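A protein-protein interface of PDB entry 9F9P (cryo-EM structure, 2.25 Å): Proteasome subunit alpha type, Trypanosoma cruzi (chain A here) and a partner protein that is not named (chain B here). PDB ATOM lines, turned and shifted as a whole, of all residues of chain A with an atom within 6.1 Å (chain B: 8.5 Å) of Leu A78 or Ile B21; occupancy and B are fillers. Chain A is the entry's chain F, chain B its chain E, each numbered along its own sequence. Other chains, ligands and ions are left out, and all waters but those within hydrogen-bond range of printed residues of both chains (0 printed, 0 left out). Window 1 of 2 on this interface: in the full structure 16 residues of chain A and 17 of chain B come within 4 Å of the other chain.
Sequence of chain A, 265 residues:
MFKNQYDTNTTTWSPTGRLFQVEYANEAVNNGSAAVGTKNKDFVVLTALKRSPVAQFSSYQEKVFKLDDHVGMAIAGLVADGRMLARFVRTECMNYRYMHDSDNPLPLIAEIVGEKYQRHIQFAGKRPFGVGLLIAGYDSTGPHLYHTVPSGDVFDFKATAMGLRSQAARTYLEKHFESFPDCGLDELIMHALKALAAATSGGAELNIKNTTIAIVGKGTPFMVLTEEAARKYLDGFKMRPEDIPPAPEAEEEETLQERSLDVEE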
ATOM      1  N   ALA A  28      -7.642  15.764 -23.717  1.00  0.00           N
ATOM      2  CA  ALA A  28      -7.425  14.332 -23.745  1.00  0.00           C
ATOM      3  C   ALA A  28      -6.214  13.991 -24.604  1.00  0.00           C
ATOM      4  O   ALA A  28      -5.489  13.054 -24.307  1.00  0.00           O
ATOM      5  CB  ALA A  28      -8.654  13.636 -24.290  1.00  0.00           C
ATOM      6  N   ILE A  75      -1.866   7.128 -32.674  1.00  0.00           N
ATOM      7  CA  ILE A  75      -2.872   7.861 -31.926  1.00  0.00           C
ATOM      8  C   ILE A  75      -2.352   8.382 -30.585  1.00  0.00           C
ATOM      9  O   ILE A  75      -1.316   7.915 -30.127  1.00  0.00           O
ATOM     10  CB  ILE A  75      -4.092   6.975 -31.702  1.00  0.00           C
ATOM     11  CG1 ILE A  75      -3.805   5.921 -30.651  1.00  0.00           C
ATOM     12  CG2 ILE A  75      -4.574   6.376 -33.016  1.00  0.00           C
ATOM     13  CD1 ILE A  75      -4.970   4.961 -30.487  1.00  0.00           C
ATOM     14  N   ALA A  76      -3.068   9.375 -30.013  1.00  0.00           N
ATOM     15  CA  ALA A  76      -2.888   9.863 -28.648  1.00  0.00           C
ATOM     16  C   ALA A  76      -4.228  10.289 -28.047  1.00  0.00           C
ATOM     17  O   ALA A  76      -4.951  11.039 -28.688  1.00  0.00           O
ATOM     18  CB  ALA A  76      -1.939  11.021 -28.601  1.00  0.00           C
ATOM     19  N   GLY A  77      -4.548   9.820 -26.831  1.00  0.00           N
ATOM     20  CA  GLY A  77      -5.810  10.110 -26.164  1.00  0.00           C
ATOM     21  C   GLY A  77      -6.627   8.845 -25.933  1.00  0.00           C
ATOM     22  O   GLY A  77      -6.068   7.795 -25.681  1.00  0.00           O
ATOM     23  N   LEU A  78      -7.937   8.897 -26.123  1.00  0.00           N
ATOM     24  CA  LEU A  78      -8.772   7.747 -25.839  1.00  0.00           C
ATOM     25  C   LEU A  78      -8.634   6.654 -26.901  1.00  0.00           C
ATOM     26  O   LEU A  78      -9.088   6.794 -28.026  1.00  0.00           O
ATOM     27  CB  LEU A  78     -10.228   8.215 -25.741  1.00  0.00           C
ATOM     28  CG  LEU A  78     -10.512   9.369 -24.765  1.00  0.00           C
ATOM     29  CD1 LEU A  78     -12.020   9.472 -24.528  1.00  0.00           C
ATOM     30  CD2 LEU A  78      -9.759   9.217 -23.431  1.00  0.00           C
ATOM     31  N   VAL A  79      -8.114   5.498 -26.495  1.00  0.00           N
ATOM     32  CA  VAL A  79      -7.908   4.385 -27.408  1.00  0.00           C
ATOM     33  C   VAL A  79      -9.209   3.872 -28.021  1.00  0.00           C
ATOM     34  O   VAL A  79      -9.213   3.486 -29.185  1.00  0.00           O
ATOM     35  CB  VAL A  79      -7.157   3.229 -26.735  1.00  0.00           C
ATOM     36  CG1 VAL A  79      -6.699   2.224 -27.780  1.00  0.00           C
ATOM     37  CG2 VAL A  79      -5.967   3.742 -25.930  1.00  0.00           C
ATOM     38  N   ALA A  80     -10.320   3.821 -27.295  1.00  0.00           N
ATOM     39  CA  ALA A  80     -11.494   3.241 -27.923  1.00  0.00           C
ATOM     40  C   ALA A  80     -12.011   4.138 -29.058  1.00  0.00           C
ATOM     41  O   ALA A  80     -12.590   3.606 -30.018  1.00  0.00           O
ATOM     42  CB  ALA A  80     -12.600   2.922 -26.948  1.00  0.00           C
ATOM     43  N   ASP A  81     -11.738   5.456 -28.996  1.00  0.00           N
ATOM     44  CA  ASP A  81     -12.085   6.350 -30.090  1.00  0.00           C
ATOM     45  C   ASP A  81     -11.111   6.161 -31.261  1.00  0.00           C
ATOM     46  O   ASP A  81     -11.523   6.180 -32.400  1.00  0.00           O
ATOM     47  CB  ASP A  81     -12.098   7.810 -29.632  1.00  0.00           C
ATOM     48  CG  ASP A  81     -13.207   8.236 -28.676  1.00  0.00           C
ATOM     49  OD1 ASP A  81     -14.050   7.376 -28.293  1.00  0.00           O
ATOM     50  OD2 ASP A  81     -13.225   9.444 -28.306  1.00  0.00           O
ATOM     51  N   GLY A  82      -9.814   5.997 -30.964  1.00  0.00           N
ATOM     52  CA  GLY A  82      -8.810   5.604 -31.939  1.00  0.00           C
ATOM     53  C   GLY A  82      -9.268   4.429 -32.805  1.00  0.00           C
ATOM     54  O   GLY A  82      -9.234   4.543 -34.030  1.00  0.00           O
ATOM     55  N   ARG A  83      -9.733   3.350 -32.156  1.00  0.00           N
ATOM     56  CA  ARG A  83     -10.143   2.130 -32.830  1.00  0.00           C
ATOM     57  C   ARG A  83     -11.364   2.352 -33.716  1.00  0.00           C
ATOM     58  O   ARG A  83     -11.458   1.754 -34.785  1.00  0.00           O
ATOM     59  CB  ARG A  83     -10.520   1.002 -31.852  1.00  0.00           C
ATOM     60  CG  ARG A  83      -9.344   0.349 -31.136  1.00  0.00           C
ATOM     61  CD  ARG A  83      -9.717  -1.073 -30.731  1.00  0.00           C
ATOM     62  NE  ARG A  83     -10.782  -1.107 -29.740  1.00  0.00           N
ATOM     63  CZ  ARG A  83     -10.612  -0.878 -28.432  1.00  0.00           C
ATOM     64  NH1 ARG A  83     -11.677  -0.828 -27.642  1.00  0.00           N
ATOM     65  NH2 ARG A  83      -9.399  -0.686 -27.930  1.00  0.00           N
ATOM     66  N   ARG A 127     -21.007  12.812 -28.897  1.00  0.00           N
ATOM     67  CA  ARG A 127     -19.889  13.258 -28.058  1.00  0.00           C
ATOM     68  C   ARG A 127     -18.698  13.575 -28.976  1.00  0.00           C
ATOM     69  O   ARG A 127     -18.458  12.849 -29.945  1.00  0.00           O
ATOM     70  CB  ARG A 127     -19.578  12.058 -27.134  1.00  0.00           C
ATOM     71  CG  ARG A 127     -18.359  12.213 -26.239  1.00  0.00           C
ATOM     72  CD  ARG A 127     -18.206  11.027 -25.311  1.00  0.00           C
ATOM     73  NE  ARG A 127     -17.867   9.742 -25.919  1.00  0.00           N
ATOM     74  CZ  ARG A 127     -16.665   9.391 -26.390  1.00  0.00           C
ATOM     75  NH1 ARG A 127     -15.697  10.275 -26.597  1.00  0.00           N
ATOM     76  NH2 ARG A 127     -16.451   8.125 -26.708  1.00  0.00           N
ATOM     77  N   PRO A 128     -17.880  14.593 -28.713  1.00  0.00           N
ATOM     78  CA  PRO A 128     -16.620  14.749 -29.430  1.00  0.00           C
ATOM     79  C   PRO A 128     -15.709  13.533 -29.284  1.00  0.00           C
ATOM     80  O   PRO A 128     -15.768  12.829 -28.292  1.00  0.00           O
ATOM     81  CB  PRO A 128     -15.961  15.986 -28.830  1.00  0.00           C
ATOM     82  CG  PRO A 128     -17.066  16.694 -28.060  1.00  0.00           C
ATOM     83  CD  PRO A 128     -18.118  15.640 -27.746  1.00  0.00           C
ATOM     84  N   PHE A 129     -14.933  13.239 -30.328  1.00  0.00           N
ATOM     85  CA  PHE A 129     -13.846  12.269 -30.248  1.00  0.00           C
ATOM     86  C   PHE A 129     -12.685  12.847 -29.462  1.00  0.00           C
ATOM     87  O   PHE A 129     -12.146  13.873 -29.848  1.00  0.00           O
ATOM     88  CB  PHE A 129     -13.284  11.932 -31.630  1.00  0.00           C
ATOM     89  CG  PHE A 129     -14.225  11.122 -32.473  1.00  0.00           C
ATOM     90  CD1 PHE A 129     -14.429   9.788 -32.200  1.00  0.00           C
ATOM     91  CD2 PHE A 129     -14.919  11.697 -33.519  1.00  0.00           C
ATOM     92  CE1 PHE A 129     -15.309   9.028 -32.966  1.00  0.00           C
ATOM     93  CE2 PHE A 129     -15.775  10.943 -34.306  1.00  0.00           C
ATOM     94  CZ  PHE A 129     -15.990   9.616 -34.017  1.00  0.00           C
ATOM     95  N   GLY A 130     -12.225  12.133 -28.445  1.00  0.00           N
ATOM     96  CA  GLY A 130     -11.119  12.617 -27.645  1.00  0.00           C
ATOM     97  C   GLY A 130      -9.785  12.026 -28.057  1.00  0.00           C
ATOM     98  O   GLY A 130      -9.022  11.659 -27.189  1.00  0.00           O
ATOM     99  N   VAL A 131      -9.431  12.078 -29.351  1.00  0.00           N
ATOM    100  CA  VAL A 131      -8.208  11.444 -29.830  1.00  0.00           C
ATOM    101  C   VAL A 131      -7.584  12.262 -30.949  1.00  0.00           C
ATOM    102  O   VAL A 131      -8.298  12.876 -31.731  1.00  0.00           O
ATOM    103  CB  VAL A 131      -8.550  10.008 -30.264  1.00  0.00           C
ATOM    104  CG1 VAL A 131      -9.259   9.941 -31.598  1.00  0.00           C
ATOM    105  CG2 VAL A 131      -7.328   9.142 -30.321  1.00  0.00           C
ATOM    106  N   ARG B  10     -25.297  17.171 -15.341  1.00  0.00           N
ATOM    107  CA  ARG B  10     -24.404  17.141 -16.488  1.00  0.00           C
ATOM    108  C   ARG B  10     -24.445  15.756 -17.145  1.00  0.00           C
ATOM    109  O   ARG B  10     -24.340  14.732 -16.480  1.00  0.00           O
ATOM    110  CB  ARG B  10     -22.988  17.545 -16.080  1.00  0.00           C
ATOM    111  CG  ARG B  10     -22.230  16.491 -15.297  1.00  0.00           C
ATOM    112  CD  ARG B  10     -20.791  16.917 -15.195  1.00  0.00           C
ATOM    113  NE  ARG B  10     -20.490  17.978 -14.245  1.00  0.00           N
ATOM    114  CZ  ARG B  10     -19.736  17.794 -13.163  1.00  0.00           C
ATOM    115  NH1 ARG B  10     -19.564  16.571 -12.682  1.00  0.00           N
ATOM    116  NH2 ARG B  10     -19.191  18.829 -12.547  1.00  0.00           N
ATOM    117  N   GLY B  11     -24.578  15.764 -18.471  1.00  0.00           N
ATOM    118  CA  GLY B  11     -24.958  14.606 -19.252  1.00  0.00           C
ATOM    119  C   GLY B  11     -23.897  13.508 -19.313  1.00  0.00           C
ATOM    120  O   GLY B  11     -22.762  13.659 -18.851  1.00  0.00           O
ATOM    121  N   VAL B  12     -24.306  12.413 -19.954  1.00  0.00           N
ATOM    122  CA  VAL B  12     -23.599  11.146 -19.956  1.00  0.00           C
ATOM    123  C   VAL B  12     -22.330  11.214 -20.822  1.00  0.00           C
ATOM    124  O   VAL B  12     -21.370  10.498 -20.562  1.00  0.00           O
ATOM    125  CB  VAL B  12     -24.624  10.067 -20.388  1.00  0.00           C
ATOM    126  CG1 VAL B  12     -24.029   8.880 -21.123  1.00  0.00           C
ATOM    127  CG2 VAL B  12     -25.417   9.561 -19.187  1.00  0.00           C
ATOM    128  N   ASN B  13     -22.308  12.130 -21.798  1.00  0.00           N
ATOM    129  CA  ASN B  13     -21.236  12.329 -22.768  1.00  0.00           C
ATOM    130  C   ASN B  13     -20.267  13.463 -22.401  1.00  0.00           C
ATOM    131  O   ASN B  13     -19.487  13.901 -23.223  1.00  0.00           O
ATOM    132  CB  ASN B  13     -21.840  12.755 -24.119  1.00  0.00           C
ATOM    133  CG  ASN B  13     -22.517  11.622 -24.887  1.00  0.00           C
ATOM    134  OD1 ASN B  13     -22.215  10.435 -24.699  1.00  0.00           O
ATOM    135  ND2 ASN B  13     -23.396  11.995 -25.804  1.00  0.00           N
ATOM    136  N   THR B  14     -20.309  13.999 -21.203  1.00  0.00           N
ATOM    137  CA  THR B  14     -19.550  15.188 -20.901  1.00  0.00           C
ATOM    138  C   THR B  14     -18.097  14.860 -20.573  1.00  0.00           C
ATOM    139  O   THR B  14     -17.855  13.923 -19.825  1.00  0.00           O
ATOM    140  CB  THR B  14     -20.263  15.891 -19.751  1.00  0.00           C
ATOM    141  OG1 THR B  14     -21.578  16.132 -20.234  1.00  0.00           O
ATOM    142  CG2 THR B  14     -19.605  17.168 -19.308  1.00  0.00           C
ATOM    143  N   PHE B  15     -17.173  15.686 -21.071  1.00  0.00           N
ATOM    144  CA  PHE B  15     -15.779  15.692 -20.680  1.00  0.00           C
ATOM    145  C   PHE B  15     -15.538  16.642 -19.532  1.00  0.00           C
ATOM    146  O   PHE B  15     -16.161  17.684 -19.465  1.00  0.00           O
ATOM    147  CB  PHE B  15     -14.855  16.227 -21.774  1.00  0.00           C
ATOM    148  CG  PHE B  15     -14.522  15.276 -22.887  1.00  0.00           C
ATOM    149  CD1 PHE B  15     -13.425  14.436 -22.795  1.00  0.00           C
ATOM    150  CD2 PHE B  15     -15.347  15.164 -23.989  1.00  0.00           C
ATOM    151  CE1 PHE B  15     -13.129  13.512 -23.786  1.00  0.00           C
ATOM    152  CE2 PHE B  15     -15.057  14.241 -24.996  1.00  0.00           C
ATOM    153  CZ  PHE B  15     -13.925  13.433 -24.914  1.00  0.00           C
ATOM    154  N   SER B  16     -14.629  16.244 -18.630  1.00  0.00           N
ATOM    155  CA  SER B  16     -14.109  17.078 -17.544  1.00  0.00           C
ATOM    156  C   SER B  16     -13.060  18.021 -18.098  1.00  0.00           C
ATOM    157  O   SER B  16     -12.670  17.833 -19.230  1.00  0.00           O
ATOM    158  CB  SER B  16     -13.503  16.222 -16.437  1.00  0.00           C
ATOM    159  OG  SER B  16     -12.226  15.685 -16.790  1.00  0.00           O
ATOM    160  N   PRO B  17     -12.602  19.061 -17.376  1.00  0.00           N
ATOM    161  CA  PRO B  17     -11.557  19.967 -17.889  1.00  0.00           C
ATOM    162  C   PRO B  17     -10.142  19.411 -18.062  1.00  0.00           C
ATOM    163  O   PRO B  17      -9.325  20.053 -18.713  1.00  0.00           O
ATOM    164  CB  PRO B  17     -11.511  21.126 -16.865  1.00  0.00           C
ATOM    165  CG  PRO B  17     -12.869  21.046 -16.177  1.00  0.00           C
ATOM    166  CD  PRO B  17     -13.200  19.556 -16.132  1.00  0.00           C
ATOM    167  N   GLU B  18      -9.843  18.220 -17.545  1.00  0.00           N
ATOM    168  CA  GLU B  18      -8.552  17.595 -17.827  1.00  0.00           C
ATOM    169  C   GLU B  18      -8.726  16.475 -18.852  1.00  0.00           C
ATOM    170  O   GLU B  18      -7.815  15.681 -19.079  1.00  0.00           O
ATOM    171  CB  GLU B  18      -7.843  17.111 -16.553  1.00  0.00           C
ATOM    172  CG  GLU B  18      -8.785  16.551 -15.492  1.00  0.00           C
ATOM    173  CD  GLU B  18      -9.496  17.570 -14.607  1.00  0.00           C
ATOM    174  OE1 GLU B  18      -8.966  18.692 -14.452  1.00  0.00           O
ATOM    175  OE2 GLU B  18     -10.595  17.242 -14.095  1.00  0.00           O
ATOM    176  N   GLY B  19      -9.901  16.398 -19.471  1.00  0.00           N
ATOM    177  CA  GLY B  19     -10.048  15.597 -20.675  1.00  0.00           C
ATOM    178  C   GLY B  19     -10.534  14.171 -20.440  1.00  0.00           C
ATOM    179  O   GLY B  19     -10.446  13.360 -21.338  1.00  0.00           O
ATOM    180  N   ARG B  20     -11.096  13.885 -19.262  1.00  0.00           N
ATOM    181  CA  ARG B  20     -11.672  12.577 -18.985  1.00  0.00           C
ATOM    182  C   ARG B  20     -13.196  12.632 -19.055  1.00  0.00           C
ATOM    183  O   ARG B  20     -13.793  13.668 -18.815  1.00  0.00           O
ATOM    184  CB  ARG B  20     -11.192  12.153 -17.609  1.00  0.00           C
ATOM    185  CG  ARG B  20      -9.728  11.758 -17.602  1.00  0.00           C
ATOM    186  CD  ARG B  20      -9.141  12.128 -16.266  1.00  0.00           C
ATOM    187  NE  ARG B  20      -8.010  11.291 -15.899  1.00  0.00           N
ATOM    188  CZ  ARG B  20      -7.542  11.188 -14.658  1.00  0.00           C
ATOM    189  NH1 ARG B  20      -8.068  11.924 -13.692  1.00  0.00           N
ATOM    190  NH2 ARG B  20      -6.556  10.349 -14.384  1.00  0.00           N
ATOM    191  N   ILE B  21     -13.798  11.525 -19.456  1.00  0.00           N
ATOM    192  CA  ILE B  21     -15.243  11.360 -19.463  1.00  0.00           C
ATOM    193  C   ILE B  21     -15.698  10.936 -18.064  1.00  0.00           C
ATOM    194  O   ILE B  21     -15.230   9.914 -17.558  1.00  0.00           O
ATOM    195  CB  ILE B  21     -15.581  10.294 -20.520  1.00  0.00           C
ATOM    196  CG1 ILE B  21     -14.996  10.696 -21.873  1.00  0.00           C
ATOM    197  CG2 ILE B  21     -17.075  10.003 -20.584  1.00  0.00           C
ATOM    198  CD1 ILE B  21     -15.539   9.920 -23.033  1.00  0.00           C
ATOM    199  N   PHE B  22     -16.555  11.740 -17.425  1.00  0.00           N
ATOM    200  CA  PHE B  22     -16.938  11.549 -16.023  1.00  0.00           C
ATOM    201  C   PHE B  22     -17.548  10.170 -15.719  1.00  0.00           C
ATOM    202  O   PHE B  22     -17.181   9.533 -14.759  1.00  0.00           O
ATOM    203  CB  PHE B  22     -17.964  12.617 -15.640  1.00  0.00           C
ATOM    204  CG  PHE B  22     -17.410  13.994 -15.340  1.00  0.00           C
ATOM    205  CD1 PHE B  22     -16.499  14.188 -14.296  1.00  0.00           C
ATOM    206  CD2 PHE B  22     -17.844  15.107 -16.061  1.00  0.00           C
ATOM    207  CE1 PHE B  22     -16.016  15.456 -13.999  1.00  0.00           C
ATOM    208  CE2 PHE B  22     -17.363  16.378 -15.765  1.00  0.00           C
ATOM    209  CZ  PHE B  22     -16.452  16.550 -14.732  1.00  0.00           C
ATOM    210  N   GLN B  23     -18.499   9.703 -16.524  1.00  0.00           N
ATOM    211  CA  GLN B  23     -19.124   8.417 -16.265  1.00  0.00           C
ATOM    212  C   GLN B  23     -18.121   7.264 -16.303  1.00  0.00           C
ATOM    213  O   GLN B  23     -18.351   6.234 -15.687  1.00  0.00           O
ATOM    214  CB  GLN B  23     -20.170   8.067 -17.323  1.00  0.00           C
ATOM    215  CG  GLN B  23     -21.485   8.828 -17.217  1.00  0.00           C
ATOM    216  CD  GLN B  23     -22.226   8.523 -15.938  1.00  0.00           C
ATOM    217  OE1 GLN B  23     -22.833   7.469 -15.783  1.00  0.00           O
ATOM    218  NE2 GLN B  23     -22.176   9.465 -15.019  1.00  0.00           N
ATOM    219  N   ILE B  24     -17.048   7.389 -17.086  1.00  0.00           N
ATOM    220  CA  ILE B  24     -16.024   6.357 -17.138  1.00  0.00           C
ATOM    221  C   ILE B  24     -15.149   6.414 -15.896  1.00  0.00           C
ATOM    222  O   ILE B  24     -14.810   5.375 -15.370  1.00  0.00           O
ATOM    223  CB  ILE B  24     -15.244   6.427 -18.456  1.00  0.00           C
ATOM    224  CG1 ILE B  24     -16.133   5.932 -19.596  1.00  0.00           C
ATOM    225  CG2 ILE B  24     -13.969   5.617 -18.371  1.00  0.00           C
ATOM    226  CD1 ILE B  24     -15.560   6.148 -20.979  1.00  0.00           C
ATOM    227  N   GLU B  25     -14.904   7.588 -15.335  1.00  0.00           N
ATOM    228  CA  GLU B  25     -14.114   7.690 -14.119  1.00  0.00           C
ATOM    229  C   GLU B  25     -14.862   7.109 -12.927  1.00  0.00           C
ATOM    230  O   GLU B  25     -14.285   6.435 -12.083  1.00  0.00           O
ATOM    231  CB  GLU B  25     -13.739   9.146 -13.878  1.00  0.00           C
ATOM    232  CG  GLU B  25     -12.833   9.689 -14.988  1.00  0.00           C
ATOM    233  CD  GLU B  25     -11.464   9.001 -15.113  1.00  0.00           C
ATOM    234  OE1 GLU B  25     -10.604   9.227 -14.220  1.00  0.00           O
ATOM    235  OE2 GLU B  25     -11.247   8.219 -16.094  1.00  0.00           O
ATOM    236  N   TYR B  26     -16.162   7.323 -12.883  1.00  0.00           N
ATOM    237  CA  TYR B  26     -16.973   6.817 -11.793  1.00  0.00           C
ATOM    238  C   TYR B  26     -17.139   5.299 -11.885  1.00  0.00           C
ATOM    239  O   TYR B  26     -17.110   4.595 -10.886  1.00  0.00           O
ATOM    240  CB  TYR B  26     -18.337   7.508 -11.842  1.00  0.00           C
ATOM    241  CG  TYR B  26     -18.340   9.017 -11.743  1.00  0.00           C
ATOM    242  CD1 TYR B  26     -17.298   9.726 -11.172  1.00  0.00           C
ATOM    243  CD2 TYR B  26     -19.427   9.746 -12.219  1.00  0.00           C
ATOM    244  CE1 TYR B  26     -17.340  11.108 -11.075  1.00  0.00           C
ATOM    245  CE2 TYR B  26     -19.490  11.136 -12.117  1.00  0.00           C
ATOM    246  CZ  TYR B  26     -18.443  11.820 -11.538  1.00  0.00           C
ATOM    247  OH  TYR B  26     -18.523  13.194 -11.468  1.00  0.00           O
ATOM    248  N   ALA B  27     -17.363   4.778 -13.089  1.00  0.00           N
ATOM    249  CA  ALA B  27     -17.399   3.332 -13.259  1.00  0.00           C
ATOM    250  C   ALA B  27     -16.123   2.669 -12.747  1.00  0.00           C
ATOM    251  O   ALA B  27     -16.201   1.639 -12.098  1.00  0.00           O
ATOM    252  CB  ALA B  27     -17.645   2.990 -14.701  1.00  0.00           C
ATOM    253  N   ILE B  28     -14.957   3.291 -12.933  1.00  0.00           N
ATOM    254  CA  ILE B  28     -13.700   2.756 -12.422  1.00  0.00           C
ATOM    255  C   ILE B  28     -13.645   2.815 -10.904  1.00  0.00           C
ATOM    256  O   ILE B  28     -13.021   1.961 -10.295  1.00  0.00           O
ATOM    257  CB  ILE B  28     -12.489   3.463 -13.087  1.00  0.00           C
ATOM    258  CG1 ILE B  28     -12.361   3.006 -14.544  1.00  0.00           C
ATOM    259  CG2 ILE B  28     -11.173   3.245 -12.342  1.00  0.00           C
ATOM    260  CD1 ILE B  28     -11.577   3.946 -15.388  1.00  0.00           C
ATOM    261  N   VAL B 121     -18.344  -0.166 -24.824  1.00  0.00           N
ATOM    262  CA  VAL B 121     -18.119   1.252 -25.120  1.00  0.00           C
ATOM    263  C   VAL B 121     -19.316   1.882 -25.858  1.00  0.00           C
ATOM    264  O   VAL B 121     -19.352   3.093 -26.093  1.00  0.00           O
ATOM    265  CB  VAL B 121     -16.796   1.381 -25.910  1.00  0.00           C
ATOM    266  CG1 VAL B 121     -16.716   2.607 -26.808  1.00  0.00           C
ATOM    267  CG2 VAL B 121     -15.607   1.359 -24.963  1.00  0.00           C
ATOM    268  N   PHE B 123     -22.302   3.307 -25.305  1.00  0.00           N
ATOM    269  CA  PHE B 123     -23.255   4.041 -24.474  1.00  0.00           C
ATOM    270  C   PHE B 123     -23.272   5.514 -24.876  1.00  0.00           C
ATOM    271  O   PHE B 123     -22.291   5.971 -25.436  1.00  0.00           O
ATOM    272  CB  PHE B 123     -22.915   3.904 -22.977  1.00  0.00           C
ATOM    273  CG  PHE B 123     -21.698   4.679 -22.527  1.00  0.00           C
ATOM    274  CD1 PHE B 123     -21.836   5.920 -21.912  1.00  0.00           C
ATOM    275  CD2 PHE B 123     -20.423   4.166 -22.728  1.00  0.00           C
ATOM    276  CE1 PHE B 123     -20.719   6.658 -21.545  1.00  0.00           C
ATOM    277  CE2 PHE B 123     -19.307   4.901 -22.359  1.00  0.00           C
ATOM    278  CZ  PHE B 123     -19.457   6.138 -21.764  1.00  0.00           C
ATOM    279  N   PRO B 136     -21.849   3.156 -18.878  1.00  0.00           N
ATOM    280  CA  PRO B 136     -20.870   2.089 -19.097  1.00  0.00           C
ATOM    281  C   PRO B 136     -21.058   0.888 -18.185  1.00  0.00           C
ATOM    282  O   PRO B 136     -21.752   1.020 -17.184  1.00  0.00           O
ATOM    283  CB  PRO B 136     -19.541   2.787 -18.772  1.00  0.00           C
ATOM    284  CG  PRO B 136     -19.888   3.933 -17.883  1.00  0.00           C
ATOM    285  CD  PRO B 136     -21.222   4.393 -18.399  1.00  0.00           C
ATOM    286  N   SER B 159     -13.230   1.812 -19.851  1.00  0.00           N
ATOM    287  CA  SER B 159     -12.787   2.641 -20.971  1.00  0.00           C
ATOM    288  C   SER B 159     -12.616   1.902 -22.301  1.00  0.00           C
ATOM    289  O   SER B 159     -12.195   2.528 -23.266  1.00  0.00           O
ATOM    290  CB  SER B 159     -11.492   3.318 -20.647  1.00  0.00           C
ATOM    291  OG  SER B 159     -10.633   2.482 -19.890  1.00  0.00           O
ATOM    292  N   GLY B 160     -12.904   0.597 -22.374  1.00  0.00           N
ATOM    293  CA  GLY B 160     -12.629  -0.208 -23.558  1.00  0.00           C
ATOM    294  C   GLY B 160     -11.139  -0.317 -23.929  1.00  0.00           C
ATOM    295  O   GLY B 160     -10.804  -0.452 -25.105  1.00  0.00           O
ATOM    296  N   THR B 161     -10.244  -0.227 -22.951  1.00  0.00           N
ATOM    297  CA  THR B 161      -8.851  -0.519 -23.217  1.00  0.00           C
ATOM    298  C   THR B 161      -8.514  -1.920 -22.724  1.00  0.00           C
ATOM    299  O   THR B 161      -9.010  -2.349 -21.690  1.00  0.00           O
ATOM    300  CB  THR B 161      -7.871   0.508 -22.631  1.00  0.00           C
ATOM    301  OG1 THR B 161      -6.901  -0.219 -21.875  1.00  0.00           O
ATOM    302  CG2 THR B 161      -8.530   1.544 -21.753  1.00  0.00           C
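Printed residues of chain A that touch a printed residue of chain B: Ala A28, Leu A78, Ala A80, Arg A83, Arg A127, Pro A128 and Gly A130. Hydrophobic or aromatic side chains of chain A within 4 Å of the printed part of chain B: Ala A28, Leu A78 and Ala A80. Among the printed residues, no Asp or Glu carboxylate lies within 4 Å of a Lys or Arg side-chain nitrogen of the other chain.
Gly B19 touches Ala A28. CD1 of Ile B21 touches CD1 of Leu A78 (3.8 Å). Val B121 touches Ala A80. Ala A80 touches Ser B159. CG of Arg A127 touches O of Asn B13, 3.6 Å away. Arg A127 touches Phe B15. Arg A127 touches Ile B21. CE2 of Phe B15 touches O of Pro A128 (3.7 Å). Gly A130 touches Phe B15.
The backbone carbonyl oxygen (O) of Gly A130 lies within hydrogen-bond range of the backbone NH (N) of Leu A78 (3.2 Å). OD1 of Asp A81 is in salt-bridge range of NH2 of Arg A127 (3.0 Å). The backbone NH (N) of Gly A130 lies within hydrogen-bond range of the side-chain carboxylate (OD2) of Asp A81, 2.9 Å away.
Leu A78 touches one residue of chain B. Of chain A, only Leu A78 (3.8 Å) and Arg A127 (3.6 Å) come within 4 Å of Ile B21. No residue of chain B comes within 4 Å of Gly A77. Of the printed residues of chain A, Gly B160 touches Arg A83. Of the printed residues of chain B, Ala A80 touches Val B121 and Ser B159. Of the printed residues of chain B, Ala A28 touches Gly B19. Printed residues of chain B within 4 Å of Arg A127: Asn B13, Phe B15 and Ile B21. The nearest printed residue of chain A that does not touch Phe B15 is Leu A78 (4.3 Å).
The guanidinium group (NH1) of Arg A83 is in hydrogen-bond range of the backbone carbonyl oxygen (O) of Gly B160 (2.7 Å).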
